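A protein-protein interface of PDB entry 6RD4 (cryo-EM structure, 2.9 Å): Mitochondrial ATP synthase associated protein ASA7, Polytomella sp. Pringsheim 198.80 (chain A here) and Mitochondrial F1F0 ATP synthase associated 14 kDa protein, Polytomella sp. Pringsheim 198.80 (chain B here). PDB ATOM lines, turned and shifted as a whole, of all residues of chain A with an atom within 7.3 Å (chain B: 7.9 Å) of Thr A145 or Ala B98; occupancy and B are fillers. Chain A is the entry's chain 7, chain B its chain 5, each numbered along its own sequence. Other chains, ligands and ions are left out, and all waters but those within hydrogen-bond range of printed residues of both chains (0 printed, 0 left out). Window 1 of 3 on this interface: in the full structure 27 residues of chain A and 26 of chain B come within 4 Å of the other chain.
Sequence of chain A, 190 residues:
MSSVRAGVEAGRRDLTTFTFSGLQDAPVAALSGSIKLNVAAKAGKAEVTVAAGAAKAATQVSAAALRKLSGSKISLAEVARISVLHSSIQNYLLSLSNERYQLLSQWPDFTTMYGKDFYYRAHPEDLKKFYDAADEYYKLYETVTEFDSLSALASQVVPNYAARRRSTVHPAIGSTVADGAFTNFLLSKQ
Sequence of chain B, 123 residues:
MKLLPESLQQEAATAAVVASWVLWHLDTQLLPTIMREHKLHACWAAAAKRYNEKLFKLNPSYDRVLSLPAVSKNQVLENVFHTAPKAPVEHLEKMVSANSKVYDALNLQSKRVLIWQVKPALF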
ATOM      1  N   SER A  97      -6.565 -23.300 -30.273  1.00  0.00           N
ATOM      2  CA  SER A  97      -7.903 -23.476 -29.725  1.00  0.00           C
ATOM      3  C   SER A  97      -7.879 -23.715 -28.240  1.00  0.00           C
ATOM      4  O   SER A  97      -8.861 -23.437 -27.565  1.00  0.00           O
ATOM      5  CB  SER A  97      -8.617 -24.643 -30.368  1.00  0.00           C
ATOM      6  OG  SER A  97      -9.028 -24.319 -31.660  1.00  0.00           O
ATOM      7  N   TYR A 101     -10.114 -21.723 -25.553  1.00  0.00           N
ATOM      8  CA  TYR A 101     -10.911 -22.483 -24.614  1.00  0.00           C
ATOM      9  C   TYR A 101     -10.554 -22.151 -23.179  1.00  0.00           C
ATOM     10  O   TYR A 101     -11.379 -22.326 -22.289  1.00  0.00           O
ATOM     11  CB  TYR A 101     -10.686 -23.957 -24.902  1.00  0.00           C
ATOM     12  CG  TYR A 101     -11.374 -24.966 -24.046  1.00  0.00           C
ATOM     13  CD1 TYR A 101     -12.548 -25.545 -24.451  1.00  0.00           C
ATOM     14  CD2 TYR A 101     -10.802 -25.408 -22.874  1.00  0.00           C
ATOM     15  CE1 TYR A 101     -13.141 -26.485 -23.692  1.00  0.00           C
ATOM     16  CE2 TYR A 101     -11.408 -26.320 -22.110  1.00  0.00           C
ATOM     17  CZ  TYR A 101     -12.562 -26.859 -22.529  1.00  0.00           C
ATOM     18  OH  TYR A 101     -13.134 -27.798 -21.747  1.00  0.00           O
ATOM     19  N   LEU A 104     -12.696 -19.188 -22.283  1.00  0.00           N
ATOM     20  CA  LEU A 104     -14.068 -19.576 -22.031  1.00  0.00           C
ATOM     21  C   LEU A 104     -14.198 -20.418 -20.779  1.00  0.00           C
ATOM     22  O   LEU A 104     -15.316 -20.687 -20.349  1.00  0.00           O
ATOM     23  CB  LEU A 104     -14.621 -20.357 -23.206  1.00  0.00           C
ATOM     24  CG  LEU A 104     -14.644 -19.646 -24.535  1.00  0.00           C
ATOM     25  CD1 LEU A 104     -15.304 -20.508 -25.502  1.00  0.00           C
ATOM     26  CD2 LEU A 104     -15.411 -18.407 -24.420  1.00  0.00           C
ATOM     27  N   TYR A 138     -22.872 -19.819 -25.573  1.00  0.00           N
ATOM     28  CA  TYR A 138     -23.073 -21.097 -26.222  1.00  0.00           C
ATOM     29  C   TYR A 138     -22.727 -21.027 -27.690  1.00  0.00           C
ATOM     30  O   TYR A 138     -22.476 -22.053 -28.305  1.00  0.00           O
ATOM     31  CB  TYR A 138     -24.506 -21.562 -26.053  1.00  0.00           C
ATOM     32  CG  TYR A 138     -24.906 -21.733 -24.629  1.00  0.00           C
ATOM     33  CD1 TYR A 138     -24.070 -22.343 -23.730  1.00  0.00           C
ATOM     34  CD2 TYR A 138     -26.118 -21.275 -24.181  1.00  0.00           C
ATOM     35  CE1 TYR A 138     -24.439 -22.498 -22.432  1.00  0.00           C
ATOM     36  CE2 TYR A 138     -26.486 -21.421 -22.886  1.00  0.00           C
ATOM     37  CZ  TYR A 138     -25.642 -22.029 -22.021  1.00  0.00           C
ATOM     38  OH  TYR A 138     -26.014 -22.172 -20.721  1.00  0.00           O
ATOM     39  N   LEU A 140     -20.041 -19.215 -28.722  1.00  0.00           N
ATOM     40  CA  LEU A 140     -18.589 -19.241 -28.694  1.00  0.00           C
ATOM     41  C   LEU A 140     -18.077 -20.593 -28.254  1.00  0.00           C
ATOM     42  O   LEU A 140     -17.069 -21.068 -28.766  1.00  0.00           O
ATOM     43  CB  LEU A 140     -18.057 -18.175 -27.749  1.00  0.00           C
ATOM     44  CG  LEU A 140     -18.499 -16.745 -27.936  1.00  0.00           C
ATOM     45  CD1 LEU A 140     -17.892 -15.894 -26.871  1.00  0.00           C
ATOM     46  CD2 LEU A 140     -18.109 -16.286 -29.285  1.00  0.00           C
ATOM     47  N   TYR A 141     -18.744 -21.223 -27.304  1.00  0.00           N
ATOM     48  CA  TYR A 141     -18.260 -22.484 -26.780  1.00  0.00           C
ATOM     49  C   TYR A 141     -18.533 -23.646 -27.708  1.00  0.00           C
ATOM     50  O   TYR A 141     -17.758 -24.594 -27.735  1.00  0.00           O
ATOM     51  CB  TYR A 141     -18.888 -22.754 -25.431  1.00  0.00           C
ATOM     52  CG  TYR A 141     -18.325 -23.931 -24.725  1.00  0.00           C
ATOM     53  CD1 TYR A 141     -17.112 -23.861 -24.096  1.00  0.00           C
ATOM     54  CD2 TYR A 141     -19.017 -25.114 -24.673  1.00  0.00           C
ATOM     55  CE1 TYR A 141     -16.607 -24.932 -23.449  1.00  0.00           C
ATOM     56  CE2 TYR A 141     -18.513 -26.188 -24.023  1.00  0.00           C
ATOM     57  CZ  TYR A 141     -17.315 -26.091 -23.418  1.00  0.00           C
ATOM     58  OH  TYR A 141     -16.819 -27.178 -22.777  1.00  0.00           O
ATOM     59  N   GLU A 142     -19.614 -23.616 -28.465  1.00  0.00           N
ATOM     60  CA  GLU A 142     -19.871 -24.724 -29.364  1.00  0.00           C
ATOM     61  C   GLU A 142     -19.026 -24.666 -30.613  1.00  0.00           C
ATOM     62  O   GLU A 142     -18.974 -25.652 -31.340  1.00  0.00           O
ATOM     63  CB  GLU A 142     -21.348 -24.791 -29.739  1.00  0.00           C
ATOM     64  CG  GLU A 142     -22.245 -25.209 -28.584  1.00  0.00           C
ATOM     65  CD  GLU A 142     -23.668 -25.494 -29.002  1.00  0.00           C
ATOM     66  OE1 GLU A 142     -24.197 -24.756 -29.863  1.00  0.00           O
ATOM     67  OE2 GLU A 142     -24.266 -26.449 -28.454  1.00  0.00           O
ATOM     68  N   THR A 143     -18.381 -23.545 -30.897  1.00  0.00           N
ATOM     69  CA  THR A 143     -17.482 -23.481 -32.032  1.00  0.00           C
ATOM     70  C   THR A 143     -16.023 -23.614 -31.650  1.00  0.00           C
ATOM     71  O   THR A 143     -15.217 -23.939 -32.513  1.00  0.00           O
ATOM     72  CB  THR A 143     -17.673 -22.188 -32.828  1.00  0.00           C
ATOM     73  OG1 THR A 143     -16.781 -22.204 -33.931  1.00  0.00           O
ATOM     74  CG2 THR A 143     -17.339 -21.011 -32.033  1.00  0.00           C
ATOM     75  N   VAL A 144     -15.650 -23.392 -30.396  1.00  0.00           N
ATOM     76  CA  VAL A 144     -14.262 -23.602 -30.032  1.00  0.00           C
ATOM     77  C   VAL A 144     -14.018 -25.071 -29.748  1.00  0.00           C
ATOM     78  O   VAL A 144     -12.867 -25.517 -29.782  1.00  0.00           O
ATOM     79  CB  VAL A 144     -13.845 -22.731 -28.836  1.00  0.00           C
ATOM     80  CG1 VAL A 144     -14.246 -23.342 -27.559  1.00  0.00           C
ATOM     81  CG2 VAL A 144     -12.387 -22.468 -28.845  1.00  0.00           C
ATOM     82  N   THR A 145     -15.069 -25.843 -29.513  1.00  0.00           N
ATOM     83  CA  THR A 145     -14.960 -27.268 -29.307  1.00  0.00           C
ATOM     84  C   THR A 145     -15.316 -28.032 -30.554  1.00  0.00           C
ATOM     85  O   THR A 145     -15.450 -29.246 -30.509  1.00  0.00           O
ATOM     86  CB  THR A 145     -15.827 -27.700 -28.145  1.00  0.00           C
ATOM     87  OG1 THR A 145     -17.185 -27.424 -28.451  1.00  0.00           O
ATOM     88  CG2 THR A 145     -15.465 -26.920 -26.950  1.00  0.00           C
ATOM     89  N   GLU A 146     -15.444 -27.349 -31.674  1.00  0.00           N
ATOM     90  CA  GLU A 146     -15.579 -27.988 -32.973  1.00  0.00           C
ATOM     91  C   GLU A 146     -14.172 -28.293 -33.471  1.00  0.00           C
ATOM     92  O   GLU A 146     -13.619 -27.617 -34.335  1.00  0.00           O
ATOM     93  CB  GLU A 146     -16.346 -27.078 -33.913  1.00  0.00           C
ATOM     94  CG  GLU A 146     -16.707 -27.645 -35.240  1.00  0.00           C
ATOM     95  CD  GLU A 146     -17.711 -28.732 -35.157  1.00  0.00           C
ATOM     96  OE1 GLU A 146     -18.591 -28.649 -34.288  1.00  0.00           O
ATOM     97  OE2 GLU A 146     -17.640 -29.677 -35.963  1.00  0.00           O
ATOM     98  N   PHE A 147     -13.571 -29.324 -32.890  1.00  0.00           N
ATOM     99  CA  PHE A 147     -12.204 -29.682 -33.225  1.00  0.00           C
ATOM    100  C   PHE A 147     -12.100 -30.498 -34.492  1.00  0.00           C
ATOM    101  O   PHE A 147     -10.990 -30.709 -34.974  1.00  0.00           O
ATOM    102  CB  PHE A 147     -11.562 -30.482 -32.109  1.00  0.00           C
ATOM    103  CG  PHE A 147     -11.564 -29.809 -30.793  1.00  0.00           C
ATOM    104  CD1 PHE A 147     -10.907 -28.636 -30.606  1.00  0.00           C
ATOM    105  CD2 PHE A 147     -12.199 -30.381 -29.728  1.00  0.00           C
ATOM    106  CE1 PHE A 147     -10.896 -28.048 -29.382  1.00  0.00           C
ATOM    107  CE2 PHE A 147     -12.179 -29.800 -28.516  1.00  0.00           C
ATOM    108  CZ  PHE A 147     -11.539 -28.634 -28.345  1.00  0.00           C
ATOM    109  N   ASP A 148     -13.202 -30.981 -35.041  1.00  0.00           N
ATOM    110  CA  ASP A 148     -13.178 -31.625 -36.339  1.00  0.00           C
ATOM    111  C   ASP A 148     -13.125 -30.629 -37.475  1.00  0.00           C
ATOM    112  O   ASP A 148     -13.081 -31.032 -38.635  1.00  0.00           O
ATOM    113  CB  ASP A 148     -14.397 -32.511 -36.518  1.00  0.00           C
ATOM    114  CG  ASP A 148     -14.279 -33.816 -35.786  1.00  0.00           C
ATOM    115  OD1 ASP A 148     -13.282 -34.013 -35.068  1.00  0.00           O
ATOM    116  OD2 ASP A 148     -15.190 -34.654 -35.928  1.00  0.00           O
ATOM    117  N   SER A 149     -13.143 -29.344 -37.173  1.00  0.00           N
ATOM    118  CA  SER A 149     -12.966 -28.316 -38.172  1.00  0.00           C
ATOM    119  C   SER A 149     -11.546 -27.811 -38.253  1.00  0.00           C
ATOM    120  O   SER A 149     -11.242 -27.025 -39.144  1.00  0.00           O
ATOM    121  CB  SER A 149     -13.895 -27.159 -37.883  1.00  0.00           C
ATOM    122  OG  SER A 149     -15.216 -27.571 -38.120  1.00  0.00           O
ATOM    123  N   LEU B  92     -27.690 -27.658 -19.350  1.00  0.00           N
ATOM    124  CA  LEU B  92     -27.137 -29.000 -19.385  1.00  0.00           C
ATOM    125  C   LEU B  92     -27.047 -29.499 -20.814  1.00  0.00           C
ATOM    126  O   LEU B  92     -25.956 -29.737 -21.324  1.00  0.00           O
ATOM    127  CB  LEU B  92     -27.975 -29.940 -18.525  1.00  0.00           C
ATOM    128  CG  LEU B  92     -27.439 -31.345 -18.280  1.00  0.00           C
ATOM    129  CD1 LEU B  92     -27.790 -31.773 -16.914  1.00  0.00           C
ATOM    130  CD2 LEU B  92     -28.056 -32.330 -19.210  1.00  0.00           C
ATOM    131  N   GLU B  93     -28.176 -29.591 -21.504  1.00  0.00           N
ATOM    132  CA  GLU B  93     -28.203 -30.231 -22.810  1.00  0.00           C
ATOM    133  C   GLU B  93     -27.551 -29.417 -23.916  1.00  0.00           C
ATOM    134  O   GLU B  93     -27.538 -29.876 -25.057  1.00  0.00           O
ATOM    135  CB  GLU B  93     -29.635 -30.542 -23.209  1.00  0.00           C
ATOM    136  CG  GLU B  93     -30.483 -29.332 -23.429  1.00  0.00           C
ATOM    137  CD  GLU B  93     -31.804 -29.672 -24.082  1.00  0.00           C
ATOM    138  OE1 GLU B  93     -31.929 -30.807 -24.582  1.00  0.00           O
ATOM    139  OE2 GLU B  93     -32.715 -28.818 -24.095  1.00  0.00           O
ATOM    140  N   LYS B  94     -27.033 -28.234 -23.620  1.00  0.00           N
ATOM    141  CA  LYS B  94     -26.264 -27.451 -24.570  1.00  0.00           C
ATOM    142  C   LYS B  94     -24.781 -27.509 -24.299  1.00  0.00           C
ATOM    143  O   LYS B  94     -23.992 -27.410 -25.233  1.00  0.00           O
ATOM    144  CB  LYS B  94     -26.720 -25.998 -24.537  1.00  0.00           C
ATOM    145  CG  LYS B  94     -28.129 -25.752 -24.916  1.00  0.00           C
ATOM    146  CD  LYS B  94     -28.436 -24.295 -24.915  1.00  0.00           C
ATOM    147  CE  LYS B  94     -27.753 -23.625 -26.068  1.00  0.00           C
ATOM    148  NZ  LYS B  94     -28.330 -24.050 -27.366  1.00  0.00           N
ATOM    149  N   MET B  95     -24.383 -27.664 -23.039  1.00  0.00           N
ATOM    150  CA  MET B  95     -22.984 -27.890 -22.724  1.00  0.00           C
ATOM    151  C   MET B  95     -22.614 -29.349 -22.860  1.00  0.00           C
ATOM    152  O   MET B  95     -21.454 -29.659 -23.110  1.00  0.00           O
ATOM    153  CB  MET B  95     -22.669 -27.432 -21.316  1.00  0.00           C
ATOM    154  CG  MET B  95     -22.838 -25.982 -21.094  1.00  0.00           C
ATOM    155  SD  MET B  95     -21.761 -24.936 -22.036  1.00  0.00           S
ATOM    156  CE  MET B  95     -20.377 -24.867 -20.936  1.00  0.00           C
ATOM    157  N   VAL B  96     -23.567 -30.256 -22.678  1.00  0.00           N
ATOM    158  CA  VAL B  96     -23.276 -31.677 -22.807  1.00  0.00           C
ATOM    159  C   VAL B  96     -23.012 -32.037 -24.256  1.00  0.00           C
ATOM    160  O   VAL B  96     -22.055 -32.751 -24.566  1.00  0.00           O
ATOM    161  CB  VAL B  96     -24.417 -32.502 -22.201  1.00  0.00           C
ATOM    162  CG1 VAL B  96     -24.403 -33.902 -22.712  1.00  0.00           C
ATOM    163  CG2 VAL B  96     -24.265 -32.522 -20.721  1.00  0.00           C
ATOM    164  N   SER B  97     -23.815 -31.511 -25.174  1.00  0.00           N
ATOM    165  CA  SER B  97     -23.573 -31.727 -26.589  1.00  0.00           C
ATOM    166  C   SER B  97     -22.306 -31.052 -27.077  1.00  0.00           C
ATOM    167  O   SER B  97     -21.773 -31.449 -28.111  1.00  0.00           O
ATOM    168  CB  SER B  97     -24.736 -31.210 -27.408  1.00  0.00           C
ATOM    169  OG  SER B  97     -24.705 -29.804 -27.439  1.00  0.00           O
ATOM    170  N   ALA B  98     -21.825 -30.039 -26.377  1.00  0.00           N
ATOM    171  CA  ALA B  98     -20.569 -29.414 -26.735  1.00  0.00           C
ATOM    172  C   ALA B  98     -19.391 -30.063 -26.053  1.00  0.00           C
ATOM    173  O   ALA B  98     -18.285 -30.008 -26.577  1.00  0.00           O
ATOM    174  CB  ALA B  98     -20.592 -27.932 -26.389  1.00  0.00           C
ATOM    175  N   ASN B  99     -19.586 -30.656 -24.887  1.00  0.00           N
ATOM    176  CA  ASN B  99     -18.535 -31.450 -24.288  1.00  0.00           C
ATOM    177  C   ASN B  99     -18.473 -32.849 -24.856  1.00  0.00           C
ATOM    178  O   ASN B  99     -17.487 -33.544 -24.636  1.00  0.00           O
ATOM    179  CB  ASN B  99     -18.716 -31.542 -22.789  1.00  0.00           C
ATOM    180  CG  ASN B  99     -18.557 -30.237 -22.115  1.00  0.00           C
ATOM    181  OD1 ASN B  99     -17.987 -29.318 -22.661  1.00  0.00           O
ATOM    182  ND2 ASN B  99     -19.061 -30.140 -20.904  1.00  0.00           N
ATOM    183  N   SER B 100     -19.495 -33.288 -25.577  1.00  0.00           N
ATOM    184  CA  SER B 100     -19.379 -34.545 -26.290  1.00  0.00           C
ATOM    185  C   SER B 100     -18.447 -34.426 -27.476  1.00  0.00           C
ATOM    186  O   SER B 100     -18.011 -35.444 -28.005  1.00  0.00           O
ATOM    187  CB  SER B 100     -20.732 -35.024 -26.778  1.00  0.00           C
ATOM    188  OG  SER B 100     -21.182 -34.234 -27.849  1.00  0.00           O
ATOM    189  N   LYS B 101     -18.172 -33.211 -27.935  1.00  0.00           N
ATOM    190  CA  LYS B 101     -17.131 -32.977 -28.913  1.00  0.00           C
ATOM    191  C   LYS B 101     -15.765 -32.827 -28.268  1.00  0.00           C
ATOM    192  O   LYS B 101     -14.754 -33.071 -28.917  1.00  0.00           O
ATOM    193  CB  LYS B 101     -17.467 -31.739 -29.718  1.00  0.00           C
ATOM    194  CG  LYS B 101     -18.566 -31.947 -30.709  1.00  0.00           C
ATOM    195  CD  LYS B 101     -19.475 -30.774 -30.768  1.00  0.00           C
ATOM    196  CE  LYS B 101     -18.738 -29.514 -31.053  1.00  0.00           C
ATOM    197  NZ  LYS B 101     -19.653 -28.388 -31.229  1.00  0.00           N
ATOM    198  N   VAL B 102     -15.709 -32.401 -27.012  1.00  0.00           N
ATOM    199  CA  VAL B 102     -14.471 -32.446 -26.248  1.00  0.00           C
ATOM    200  C   VAL B 102     -14.126 -33.877 -25.881  1.00  0.00           C
ATOM    201  O   VAL B 102     -12.956 -34.237 -25.774  1.00  0.00           O
ATOM    202  CB  VAL B 102     -14.599 -31.554 -25.006  1.00  0.00           C
ATOM    203  CG1 VAL B 102     -13.331 -31.448 -24.262  1.00  0.00           C
ATOM    204  CG2 VAL B 102     -14.987 -30.212 -25.412  1.00  0.00           C
ATOM    205  N   TYR B 103     -15.130 -34.720 -25.669  1.00  0.00           N
ATOM    206  CA  TYR B 103     -14.834 -36.122 -25.434  1.00  0.00           C
ATOM    207  C   TYR B 103     -14.317 -36.771 -26.691  1.00  0.00           C
ATOM    208  O   TYR B 103     -13.365 -37.544 -26.631  1.00  0.00           O
ATOM    209  CB  TYR B 103     -16.058 -36.894 -24.951  1.00  0.00           C
ATOM    210  CG  TYR B 103     -15.793 -38.374 -24.769  1.00  0.00           C
ATOM    211  CD1 TYR B 103     -15.162 -38.840 -23.654  1.00  0.00           C
ATOM    212  CD2 TYR B 103     -16.168 -39.299 -25.727  1.00  0.00           C
ATOM    213  CE1 TYR B 103     -14.924 -40.155 -23.485  1.00  0.00           C
ATOM    214  CE2 TYR B 103     -15.896 -40.615 -25.569  1.00  0.00           C
ATOM    215  CZ  TYR B 103     -15.282 -41.033 -24.445  1.00  0.00           C
ATOM    216  OH  TYR B 103     -15.016 -42.354 -24.267  1.00  0.00           O
ATOM    217  N   ASP B 104     -14.959 -36.501 -27.825  1.00  0.00           N
ATOM    218  CA  ASP B 104     -14.619 -37.183 -29.063  1.00  0.00           C
ATOM    219  C   ASP B 104     -13.200 -36.879 -29.478  1.00  0.00           C
ATOM    220  O   ASP B 104     -12.400 -37.784 -29.689  1.00  0.00           O
ATOM    221  CB  ASP B 104     -15.572 -36.777 -30.170  1.00  0.00           C
ATOM    222  CG  ASP B 104     -16.885 -37.462 -30.068  1.00  0.00           C
ATOM    223  OD1 ASP B 104     -17.053 -38.248 -29.125  1.00  0.00           O
ATOM    224  OD2 ASP B 104     -17.759 -37.214 -30.920  1.00  0.00           O
ATOM    225  N   ALA B 105     -12.846 -35.614 -29.507  1.00  0.00           N
ATOM    226  CA  ALA B 105     -11.559 -35.253 -30.047  1.00  0.00           C
ATOM    227  C   ALA B 105     -10.426 -35.520 -29.081  1.00  0.00           C
ATOM    228  O   ALA B 105      -9.303 -35.738 -29.521  1.00  0.00           O
ATOM    229  CB  ALA B 105     -11.572 -33.798 -30.436  1.00  0.00           C
ATOM    230  N   LEU B 106     -10.670 -35.529 -27.780  1.00  0.00           N
ATOM    231  CA  LEU B 106      -9.552 -35.339 -26.872  1.00  0.00           C
ATOM    232  C   LEU B 106      -9.519 -36.345 -25.741  1.00  0.00           C
ATOM    233  O   LEU B 106      -9.060 -36.020 -24.648  1.00  0.00           O
ATOM    234  CB  LEU B 106      -9.596 -33.958 -26.247  1.00  0.00           C
ATOM    235  CG  LEU B 106      -9.687 -32.712 -27.083  1.00  0.00           C
ATOM    236  CD1 LEU B 106     -10.065 -31.634 -26.159  1.00  0.00           C
ATOM    237  CD2 LEU B 106      -8.376 -32.411 -27.681  1.00  0.00           C
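OG1 of Thr A145 lies within hydrogen-bond range of O of Tyr A141, 3.0 Å away. The backbone carbonyl oxygen of Met B95 lies close to the side-chain amide nitrogen of Asn B99 (3.3 Å). O of Lys B94 lies within hydrogen-bond range of OG of Ser B97 (3.3 Å). OG of Ser B100 sits at hydrogen-bond distance from O of Ser B97.
CE of Lys B94 touches CD2 of Tyr A138, 3.4 Å away. Tyr A138 touches Met B95. Met B95 touches Tyr A141 (SD to CD2, 3.8 Å). OE2 of Glu A142 touches OG of Ser B97, at 3.5 Å. Ala B98 touches Glu A142 (CB to CG, 3.9 Å). O of Thr A145 touches CB of Lys B101, at 3.3 Å. CG2 of Thr A145 touches CG2 of Val B102 (3.7 Å). CD2 of Phe A147 touches O of Lys B101, 3.8 Å away. CD2 of Phe A147 touches CB of Ala B105 (3.5 Å). CD1 of Leu B106 touches CE2 of Phe A147, at 3.7 Å.
Of chain B, only Ala B98, Lys B101 and Val B102 come within 4 Å of Thr A145. Printed residues of chain B within 4 Å of Phe A147: Lys B101 (3.8 Å), Ala B105 (3.5 Å) and Leu B106 (3.7 Å). Asp A148 touches none of the printed residues of chain B. Ser A149 touches none of the printed residues of chain B. Printed residues of chain A within 4 Å of Ser B97: Glu A142 (3.5 Å). Ala B98 touches just these residues of chain A: Tyr A141 (3.6 Å), Glu A142 (3.9 Å) and Thr A145 (3.4 Å). Of the printed residues of chain A, Leu B106 touches Phe A147 (3.7 Å). The nearest residue of chain B that does not touch Thr A145 is Asn B99 (5.4 Å). The nearest printed residue of chain A that does not touch Ala B98 is Phe A147 (6.4 Å).
The side-chain carboxylate (OE2) of Glu A142 sits close to the backbone carbonyl oxygen (O) of Lys B94, at 3.4 Å. The backbone carbonyl oxygen of Ala B98 sits at hydrogen-bond distance from the side-chain hydroxyl of Thr A145, 3.4 Å away. The side-chain hydroxyl (OH) of Tyr A141 lies within hydrogen-bond range of the side-chain amide oxygen (OD1) of Asn B99 (2.4 Å). The side-chain amino group of Lys B101 sits at hydrogen-bond distance from the backbone carbonyl oxygen of Glu A142, at 2.8 Å. NZ of Lys B101 is in salt-bridge range of OE1 of Glu A146.
Printed residues of chain A that touch a printed residue of chain B: Tyr A138, Tyr A141, Glu A142, Thr A145, Glu A146 and Phe A147. Hydrophobic or aromatic side chains of chain A that line the printed part of chain B: Tyr A138, Tyr A141 and Phe A147. Hydrophobic or aromatic side chains of chain B within 4 Å of the printed part of chain A: Met B95, Ala B98, Val B102, Ala B105 and Leu B106. Among the printed residues, Asp or Glu carboxylates within 4 Å of a Lys or Arg side-chain nitrogen of the other chain: Glu A146 with Lys B101 (3.2 Å).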
